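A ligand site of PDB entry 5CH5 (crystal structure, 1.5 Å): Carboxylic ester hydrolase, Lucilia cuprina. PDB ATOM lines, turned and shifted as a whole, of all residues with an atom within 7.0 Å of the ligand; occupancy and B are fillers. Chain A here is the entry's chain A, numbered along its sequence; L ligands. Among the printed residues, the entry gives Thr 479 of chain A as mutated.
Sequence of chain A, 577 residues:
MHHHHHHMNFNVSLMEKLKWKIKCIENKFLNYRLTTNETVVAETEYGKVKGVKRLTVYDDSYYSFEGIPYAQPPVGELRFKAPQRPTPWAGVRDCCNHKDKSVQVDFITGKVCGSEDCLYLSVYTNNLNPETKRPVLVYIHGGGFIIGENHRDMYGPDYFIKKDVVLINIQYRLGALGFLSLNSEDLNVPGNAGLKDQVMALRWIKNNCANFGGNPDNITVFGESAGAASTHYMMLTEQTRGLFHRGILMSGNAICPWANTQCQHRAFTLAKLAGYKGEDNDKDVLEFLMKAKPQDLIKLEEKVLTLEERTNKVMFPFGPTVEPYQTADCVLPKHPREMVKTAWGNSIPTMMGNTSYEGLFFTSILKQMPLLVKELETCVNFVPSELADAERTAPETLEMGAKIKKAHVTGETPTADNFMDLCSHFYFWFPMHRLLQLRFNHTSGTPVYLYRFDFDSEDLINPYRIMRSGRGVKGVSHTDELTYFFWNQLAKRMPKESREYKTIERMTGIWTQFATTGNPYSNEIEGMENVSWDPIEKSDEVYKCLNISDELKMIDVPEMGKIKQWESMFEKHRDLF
OG of Ser 225 is covalently linked to P1 of the ligand. An oxygen (O1) of the ligand sits at hydrogen-bond distance from the backbone NH (N) of Ala 226 (2.9 Å). An oxygen (O1) of the ligand sits at hydrogen-bond distance from the backbone NH (N) of Gly 144, at 2.8 Å. O1 of the ligand is in hydrogen-bond range of N of Gly 143, at 2.9 Å.
Gly 142 touches the ligand (C to O1, 3.9 Å). CD2 of Trp 258 touches C2 of the ligand, at 3.8 Å. Met 315 touches the ligand. CZ of Phe 361 touches C4 of the ligand (3.9 Å). Tyr 464 touches the ligand. His 478 touches the ligand (NE2 to C3, 3.4 Å). Thr 479 touches the ligand (CG2 to C4, 3.8 Å). Hydrophobic or aromatic side chains within 4 Å of the ligand: Ala 226, Trp 258, Met 315, Phe 361, Tyr 464 and His 478. Of the 25 residues printed, 11 come within 4 Å of the ligand. The nearest printed residue that does not touch the ligand is Phe 316 (4.1 Å).
N of Ser 225 lies close to O of Ser 251, at 3.3 Å. A ring nitrogen (NE2) of His 478 sits at hydrogen-bond distance from the side-chain hydroxyl (OG) of Ser 225 (3.1 Å). The indole nitrogen of Trp 258 lies within hydrogen-bond range of the backbone carbonyl oxygen of Tyr 427. NE2 of His 478 lies close to OE2 of Glu 224, at 3.4 Å.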
ATOM      1  N   HIS A 141      14.102   5.956  10.040  1.00  0.00           N
ATOM      2  CA  HIS A 141      13.361   4.815   9.573  1.00  0.00           C
ATOM      3  C   HIS A 141      13.056   4.927   8.106  1.00  0.00           C
ATOM      4  O   HIS A 141      12.884   6.014   7.578  1.00  0.00           O
ATOM      5  CB  HIS A 141      12.070   4.517  10.327  1.00  0.00           C
ATOM      6  CG  HIS A 141      10.990   5.528  10.100  1.00  0.00           C
ATOM      7  ND1 HIS A 141      10.197   5.506   8.968  1.00  0.00           N
ATOM      8  CD2 HIS A 141      10.647   6.630  10.798  1.00  0.00           C
ATOM      9  CE1 HIS A 141       9.368   6.530   9.020  1.00  0.00           C
ATOM     10  NE2 HIS A 141       9.617   7.230  10.120  1.00  0.00           N
ATOM     11  N   GLY A 142      13.005   3.772   7.464  1.00  0.00           N
ATOM     12  CA  GLY A 142      12.487   3.691   6.109  1.00  0.00           C
ATOM     13  C   GLY A 142      11.026   3.372   6.045  1.00  0.00           C
ATOM     14  O   GLY A 142      10.253   3.593   6.976  1.00  0.00           O
ATOM     15  N   GLY A 143      10.556   2.935   4.862  1.00  0.00           N
ATOM     16  CA  GLY A 143       9.148   2.882   4.543  1.00  0.00           C
ATOM     17  C   GLY A 143       8.716   3.726   3.330  1.00  0.00           C
ATOM     18  O   GLY A 143       7.552   4.162   3.259  1.00  0.00           O
ATOM     19  N   GLY A 144       9.564   3.813   2.318  1.00  0.00           N
ATOM     20  CA  GLY A 144       9.251   4.457   1.069  1.00  0.00           C
ATOM     21  C   GLY A 144       8.874   5.930   1.203  1.00  0.00           C
ATOM     22  O   GLY A 144       8.369   6.523   0.231  1.00  0.00           O
ATOM     23  N   PHE A 145       9.169   6.576   2.352  1.00  0.00           N
ATOM     24  CA  PHE A 145       8.661   7.989   2.621  1.00  0.00           C
ATOM     25  C   PHE A 145       7.164   8.014   2.744  1.00  0.00           C
ATOM     26  O   PHE A 145       6.579   9.113   2.758  1.00  0.00           O
ATOM     27  CB  PHE A 145       9.174   9.045   1.590  1.00  0.00           C
ATOM     28  CG  PHE A 145      10.679   9.126   1.484  1.00  0.00           C
ATOM     29  CD1 PHE A 145      11.489   9.762   2.439  1.00  0.00           C
ATOM     30  CD2 PHE A 145      11.323   8.486   0.374  1.00  0.00           C
ATOM     31  CE1 PHE A 145      12.884   9.801   2.298  1.00  0.00           C
ATOM     32  CE2 PHE A 145      12.696   8.489   0.284  1.00  0.00           C
ATOM     33  CZ  PHE A 145      13.470   9.163   1.215  1.00  0.00           C
ATOM     34  N   ILE A 147       5.368   5.204   4.882  1.00  0.00           N
ATOM     35  CA  ILE A 147       5.064   4.536   6.160  1.00  0.00           C
ATOM     36  C   ILE A 147       6.194   4.621   7.111  1.00  0.00           C
ATOM     37  O   ILE A 147       7.334   4.969   6.712  1.00  0.00           O
ATOM     38  CB  ILE A 147       4.666   3.073   5.973  1.00  0.00           C
ATOM     39  CG1 ILE A 147       5.820   2.211   5.445  1.00  0.00           C
ATOM     40  CG2 ILE A 147       3.358   3.001   5.117  1.00  0.00           C
ATOM     41  CD1 ILE A 147       5.359   0.742   5.413  1.00  0.00           C
ATOM     42  N   GLU A 224      17.726   2.482   6.973  1.00  0.00           N
ATOM     43  CA  GLU A 224      17.519   1.438   5.996  1.00  0.00           C
ATOM     44  C   GLU A 224      16.511   1.831   4.963  1.00  0.00           C
ATOM     45  O   GLU A 224      15.511   2.418   5.296  1.00  0.00           O
ATOM     46  CB  GLU A 224      17.148   0.100   6.696  1.00  0.00           C
ATOM     47  CG  GLU A 224      17.045  -1.160   5.787  1.00  0.00           C
ATOM     48  CD  GLU A 224      15.623  -1.383   5.278  1.00  0.00           C
ATOM     49  OE1 GLU A 224      14.728  -0.657   5.724  1.00  0.00           O
ATOM     50  OE2 GLU A 224      15.465  -2.269   4.427  1.00  0.00           O
ATOM     51  N   SER A 225      16.744   1.491   3.690  1.00  0.00           N
ATOM     52  CA  SER A 225      15.870   1.751   2.586  1.00  0.00           C
ATOM     53  C   SER A 225      15.620   3.288   2.476  1.00  0.00           C
ATOM     54  O   SER A 225      16.622   3.997   2.356  1.00  0.00           O
ATOM     55  CB  SER A 225      14.603   0.905   2.692  1.00  0.00           C
ATOM     56  OG  SER A 225      13.820   0.992   1.489  1.00  0.00           O
ATOM     57  N   ALA A 226      14.402   3.813   2.605  1.00  0.00           N
ATOM     58  CA  ALA A 226      14.151   5.249   2.591  1.00  0.00           C
ATOM     59  C   ALA A 226      14.880   5.967   3.734  1.00  0.00           C
ATOM     60  O   ALA A 226      15.187   7.112   3.612  1.00  0.00           O
ATOM     61  CB  ALA A 226      12.668   5.577   2.656  1.00  0.00           C
ATOM     62  N   GLY A 227      15.176   5.285   4.821  1.00  0.00           N
ATOM     63  CA  GLY A 227      15.984   5.861   5.859  1.00  0.00           C
ATOM     64  C   GLY A 227      17.452   5.942   5.445  1.00  0.00           C
ATOM     65  O   GLY A 227      18.193   6.812   5.939  1.00  0.00           O
ATOM     66  N   ALA A 228      17.922   5.058   4.554  1.00  0.00           N
ATOM     67  CA  ALA A 228      19.294   5.166   4.014  1.00  0.00           C
ATOM     68  C   ALA A 228      19.361   6.276   2.983  1.00  0.00           C
ATOM     69  O   ALA A 228      20.308   7.063   2.982  1.00  0.00           O
ATOM     70  CB  ALA A 228      19.756   3.868   3.371  1.00  0.00           C
ATOM     71  N   SER A 251      20.924  -0.674   2.545  1.00  0.00           N
ATOM     72  CA  SER A 251      20.081  -0.916   1.424  1.00  0.00           C
ATOM     73  C   SER A 251      19.419   0.349   0.902  1.00  0.00           C
ATOM     74  O   SER A 251      18.166   0.468   0.864  1.00  0.00           O
ATOM     75  CB  SER A 251      19.058  -2.012   1.695  1.00  0.00           C
ATOM     76  OG  SER A 251      19.636  -3.214   2.186  1.00  0.00           O
ATOM     77  N   TRP A 258      14.047   4.966  -6.886  1.00  0.00           N
ATOM     78  CA  TRP A 258      12.896   5.188  -6.007  1.00  0.00           C
ATOM     79  C   TRP A 258      13.085   6.286  -5.002  1.00  0.00           C
ATOM     80  O   TRP A 258      12.179   6.586  -4.302  1.00  0.00           O
ATOM     81  CB  TRP A 258      12.575   3.903  -5.262  1.00  0.00           C
ATOM     82  CG  TRP A 258      13.738   3.287  -4.545  1.00  0.00           C
ATOM     83  CD1 TRP A 258      14.602   2.280  -5.044  1.00  0.00           C
ATOM     84  CD2 TRP A 258      14.270   3.617  -3.262  1.00  0.00           C
ATOM     85  NE1 TRP A 258      15.570   1.948  -4.136  1.00  0.00           N
ATOM     86  CE2 TRP A 258      15.434   2.762  -3.045  1.00  0.00           C
ATOM     87  CE3 TRP A 258      13.950   4.542  -2.294  1.00  0.00           C
ATOM     88  CZ2 TRP A 258      16.176   2.803  -1.878  1.00  0.00           C
ATOM     89  CZ3 TRP A 258      14.736   4.551  -1.123  1.00  0.00           C
ATOM     90  CH2 TRP A 258      15.792   3.691  -0.946  1.00  0.00           C
ATOM     91  N   ALA A 259      14.275   6.865  -4.908  1.00  0.00           N
ATOM     92  CA  ALA A 259      14.567   7.807  -3.785  1.00  0.00           C
ATOM     93  C   ALA A 259      14.265   9.261  -4.053  1.00  0.00           C
ATOM     94  O   ALA A 259      14.407  10.046  -3.172  1.00  0.00           O
ATOM     95  CB  ALA A 259      16.048   7.648  -3.349  1.00  0.00           C
ATOM     96  N   MET A 315       8.108   4.560  -8.278  1.00  0.00           N
ATOM     97  CA  MET A 315       7.571   3.766  -7.176  1.00  0.00           C
ATOM     98  C   MET A 315       6.517   4.503  -6.304  1.00  0.00           C
ATOM     99  O   MET A 315       5.550   3.879  -5.825  1.00  0.00           O
ATOM    100  CB  MET A 315       8.699   3.250  -6.332  1.00  0.00           C
ATOM    101  CG  MET A 315       8.310   2.032  -5.563  1.00  0.00           C
ATOM    102  SD  MET A 315       9.566   1.412  -4.476  1.00  0.00           S
ATOM    103  CE  MET A 315      10.413   0.229  -5.546  1.00  0.00           C
ATOM    104  N   PHE A 316       6.726   5.797  -6.028  1.00  0.00           N
ATOM    105  CA  PHE A 316       5.862   6.573  -5.140  1.00  0.00           C
ATOM    106  C   PHE A 316       5.477   7.876  -5.784  1.00  0.00           C
ATOM    107  O   PHE A 316       6.336   8.472  -6.413  1.00  0.00           O
ATOM    108  CB  PHE A 316       6.574   6.862  -3.810  1.00  0.00           C
ATOM    109  CG  PHE A 316       7.172   5.637  -3.154  1.00  0.00           C
ATOM    110  CD1 PHE A 316       6.397   4.736  -2.508  1.00  0.00           C
ATOM    111  CD2 PHE A 316       8.545   5.421  -3.203  1.00  0.00           C
ATOM    112  CE1 PHE A 316       6.985   3.595  -1.923  1.00  0.00           C
ATOM    113  CE2 PHE A 316       9.152   4.266  -2.659  1.00  0.00           C
ATOM    114  CZ  PHE A 316       8.356   3.359  -2.004  1.00  0.00           C
ATOM    115  N   PHE A 361      12.105  -9.588  -1.795  1.00  0.00           N
ATOM    116  CA  PHE A 361      11.002  -8.828  -1.219  1.00  0.00           C
ATOM    117  C   PHE A 361       9.770  -8.855  -2.091  1.00  0.00           C
ATOM    118  O   PHE A 361       8.686  -8.836  -1.567  1.00  0.00           O
ATOM    119  CB  PHE A 361      11.450  -7.373  -1.038  1.00  0.00           C
ATOM    120  CG  PHE A 361      10.558  -6.554  -0.193  1.00  0.00           C
ATOM    121  CD1 PHE A 361       9.502  -5.845  -0.719  1.00  0.00           C
ATOM    122  CD2 PHE A 361      10.774  -6.463   1.198  1.00  0.00           C
ATOM    123  CE1 PHE A 361       8.672  -5.114   0.102  1.00  0.00           C
ATOM    124  CE2 PHE A 361       9.967  -5.730   2.019  1.00  0.00           C
ATOM    125  CZ  PHE A 361       8.895  -5.047   1.460  1.00  0.00           C
ATOM    126  N   PHE A 362       9.924  -8.862  -3.401  1.00  0.00           N
ATOM    127  CA  PHE A 362       8.845  -8.818  -4.372  1.00  0.00           C
ATOM    128  C   PHE A 362       8.170 -10.142  -4.653  1.00  0.00           C
ATOM    129  O   PHE A 362       7.310 -10.161  -5.513  1.00  0.00           O
ATOM    130  CB  PHE A 362       9.305  -8.146  -5.681  1.00  0.00           C
ATOM    131  CG  PHE A 362       9.835  -6.744  -5.486  1.00  0.00           C
ATOM    132  CD1 PHE A 362       8.969  -5.690  -5.119  1.00  0.00           C
ATOM    133  CD2 PHE A 362      11.203  -6.456  -5.552  1.00  0.00           C
ATOM    134  CE1 PHE A 362       9.442  -4.401  -4.908  1.00  0.00           C
ATOM    135  CE2 PHE A 362      11.669  -5.172  -5.320  1.00  0.00           C
ATOM    136  CZ  PHE A 362      10.814  -4.152  -4.992  1.00  0.00           C
ATOM    137  N   TYR A 427      17.280  -1.583  -8.132  1.00  0.00           N
ATOM    138  CA  TYR A 427      16.902  -0.720  -6.990  1.00  0.00           C
ATOM    139  C   TYR A 427      17.995  -0.518  -5.949  1.00  0.00           C
ATOM    140  O   TYR A 427      17.908   0.472  -5.143  1.00  0.00           O
ATOM    141  CB  TYR A 427      15.660  -1.279  -6.252  1.00  0.00           C
ATOM    142  CG  TYR A 427      14.362  -1.265  -7.045  1.00  0.00           C
ATOM    143  CD1 TYR A 427      13.848  -0.085  -7.551  1.00  0.00           C
ATOM    144  CD2 TYR A 427      13.699  -2.440  -7.356  1.00  0.00           C
ATOM    145  CE1 TYR A 427      12.651  -0.080  -8.266  1.00  0.00           C
ATOM    146  CE2 TYR A 427      12.537  -2.430  -8.116  1.00  0.00           C
ATOM    147  CZ  TYR A 427      12.015  -1.240  -8.528  1.00  0.00           C
ATOM    148  OH  TYR A 427      10.821  -1.215  -9.212  1.00  0.00           O
ATOM    149  N   PHE A 428      19.055  -1.328  -5.969  1.00  0.00           N
ATOM    150  CA  PHE A 428      20.023  -1.308  -4.872  1.00  0.00           C
ATOM    151  C   PHE A 428      21.512  -1.367  -5.310  1.00  0.00           C
ATOM    152  O   PHE A 428      22.270  -0.436  -5.076  1.00  0.00           O
ATOM    153  CB  PHE A 428      19.727  -2.364  -3.789  1.00  0.00           C
ATOM    154  CG  PHE A 428      18.359  -2.239  -3.196  1.00  0.00           C
ATOM    155  CD1 PHE A 428      18.025  -1.227  -2.275  1.00  0.00           C
ATOM    156  CD2 PHE A 428      17.339  -3.089  -3.618  1.00  0.00           C
ATOM    157  CE1 PHE A 428      16.706  -1.118  -1.825  1.00  0.00           C
ATOM    158  CE2 PHE A 428      16.042  -3.016  -3.109  1.00  0.00           C
ATOM    159  CZ  PHE A 428      15.698  -2.004  -2.232  1.00  0.00           C
ATOM    160  N   TYR A 464       8.010  -6.446   8.612  1.00  0.00           N
ATOM    161  CA  TYR A 464       8.035  -6.298   7.163  1.00  0.00           C
ATOM    162  C   TYR A 464       7.865  -7.662   6.498  1.00  0.00           C
ATOM    163  O   TYR A 464       7.305  -7.719   5.400  1.00  0.00           O
ATOM    164  CB  TYR A 464       9.325  -5.675   6.684  1.00  0.00           C
ATOM    165  CG  TYR A 464       9.452  -4.175   6.764  1.00  0.00           C
ATOM    166  CD1 TYR A 464       8.722  -3.373   5.917  1.00  0.00           C
ATOM    167  CD2 TYR A 464      10.466  -3.596   7.512  1.00  0.00           C
ATOM    168  CE1 TYR A 464       8.955  -2.015   5.866  1.00  0.00           C
ATOM    169  CE2 TYR A 464      10.644  -2.221   7.529  1.00  0.00           C
ATOM    170  CZ  TYR A 464       9.867  -1.445   6.706  1.00  0.00           C
ATOM    171  OH  TYR A 464      10.087  -0.085   6.691  1.00  0.00           O
ATOM    172  N   MET A 467       4.080  -7.932   6.257  1.00  0.00           N
ATOM    173  CA  MET A 467       3.676  -7.019   5.208  1.00  0.00           C
ATOM    174  C   MET A 467       3.793  -7.611   3.846  1.00  0.00           C
ATOM    175  O   MET A 467       2.900  -7.376   3.030  1.00  0.00           O
ATOM    176  CB  MET A 467       4.561  -5.794   5.184  1.00  0.00           C
ATOM    177  CG  MET A 467       4.093  -4.774   4.168  1.00  0.00           C
ATOM    178  SD  MET A 467       5.185  -3.324   4.148  1.00  0.00           S
ATOM    179  CE  MET A 467       6.079  -3.745   2.671  1.00  0.00           C
ATOM    180  N   HIS A 478      15.546  -7.850   1.167  1.00  0.00           N
ATOM    181  CA  HIS A 478      15.385  -6.449   1.651  1.00  0.00           C
ATOM    182  C   HIS A 478      14.557  -6.456   2.966  1.00  0.00           C
ATOM    183  O   HIS A 478      13.454  -7.055   3.044  1.00  0.00           O
ATOM    184  CB  HIS A 478      14.641  -5.636   0.633  1.00  0.00           C
ATOM    185  CG  HIS A 478      14.581  -4.160   0.924  1.00  0.00           C
ATOM    186  ND1 HIS A 478      15.706  -3.382   1.006  1.00  0.00           N
ATOM    187  CD2 HIS A 478      13.535  -3.319   1.102  1.00  0.00           C
ATOM    188  CE1 HIS A 478      15.352  -2.130   1.243  1.00  0.00           C
ATOM    189  NE2 HIS A 478      14.043  -2.056   1.310  1.00  0.00           N
ATOM    190  N   THR A 479      15.120  -5.771   3.949  1.00  0.00           N
ATOM    191  CA  THR A 479      14.559  -5.507   5.319  1.00  0.00           C
ATOM    192  C   THR A 479      14.930  -6.606   6.315  1.00  0.00           C
ATOM    193  O   THR A 479      14.686  -6.449   7.480  1.00  0.00           O
ATOM    194  CB  THR A 479      13.053  -5.208   5.471  1.00  0.00           C
ATOM    195  OG1 THR A 479      12.274  -6.401   5.293  1.00  0.00           O
ATOM    196  CG2 THR A 479      12.605  -4.100   4.506  1.00  0.00           C
ATOM    197  N   LEU A 482      16.973  -5.914   9.674  1.00  0.00           N
ATOM    198  CA  LEU A 482      16.398  -5.066  10.777  1.00  0.00           C
ATOM    199  C   LEU A 482      16.114  -5.843  12.069  1.00  0.00           C
ATOM    200  O   LEU A 482      16.181  -5.301  13.173  1.00  0.00           O
ATOM    201  CB  LEU A 482      15.165  -4.275  10.347  1.00  0.00           C
ATOM    202  CG  LEU A 482      15.428  -3.190   9.312  1.00  0.00           C
ATOM    203  CD1 LEU A 482      14.130  -2.704   8.864  1.00  0.00           C
ATOM    204  CD2 LEU A 482      16.227  -2.025   9.908  1.00  0.00           C
HETATM  205  O1  LIG L   1      11.920   2.292   2.407  1.00  0.00           O
HETATM  206  P1  LIG L   1      12.272   1.184   1.473  1.00  0.00           P
HETATM  207  O2  LIG L   1      12.059   1.660  -0.083  1.00  0.00           O
HETATM  208  C1  LIG L   1      12.554   0.777  -1.109  1.00  0.00           C
HETATM  209  C2  LIG L   1      11.675   0.992  -2.212  1.00  0.00           C
HETATM  210  O3  LIG L   1      11.260   0.113   1.754  1.00  0.00           O
HETATM  211  C3  LIG L   1      11.399  -0.603   2.914  1.00  0.00           C
HETATM  212  C4  LIG L   1      10.235  -1.615   2.813  1.00  0.00           C
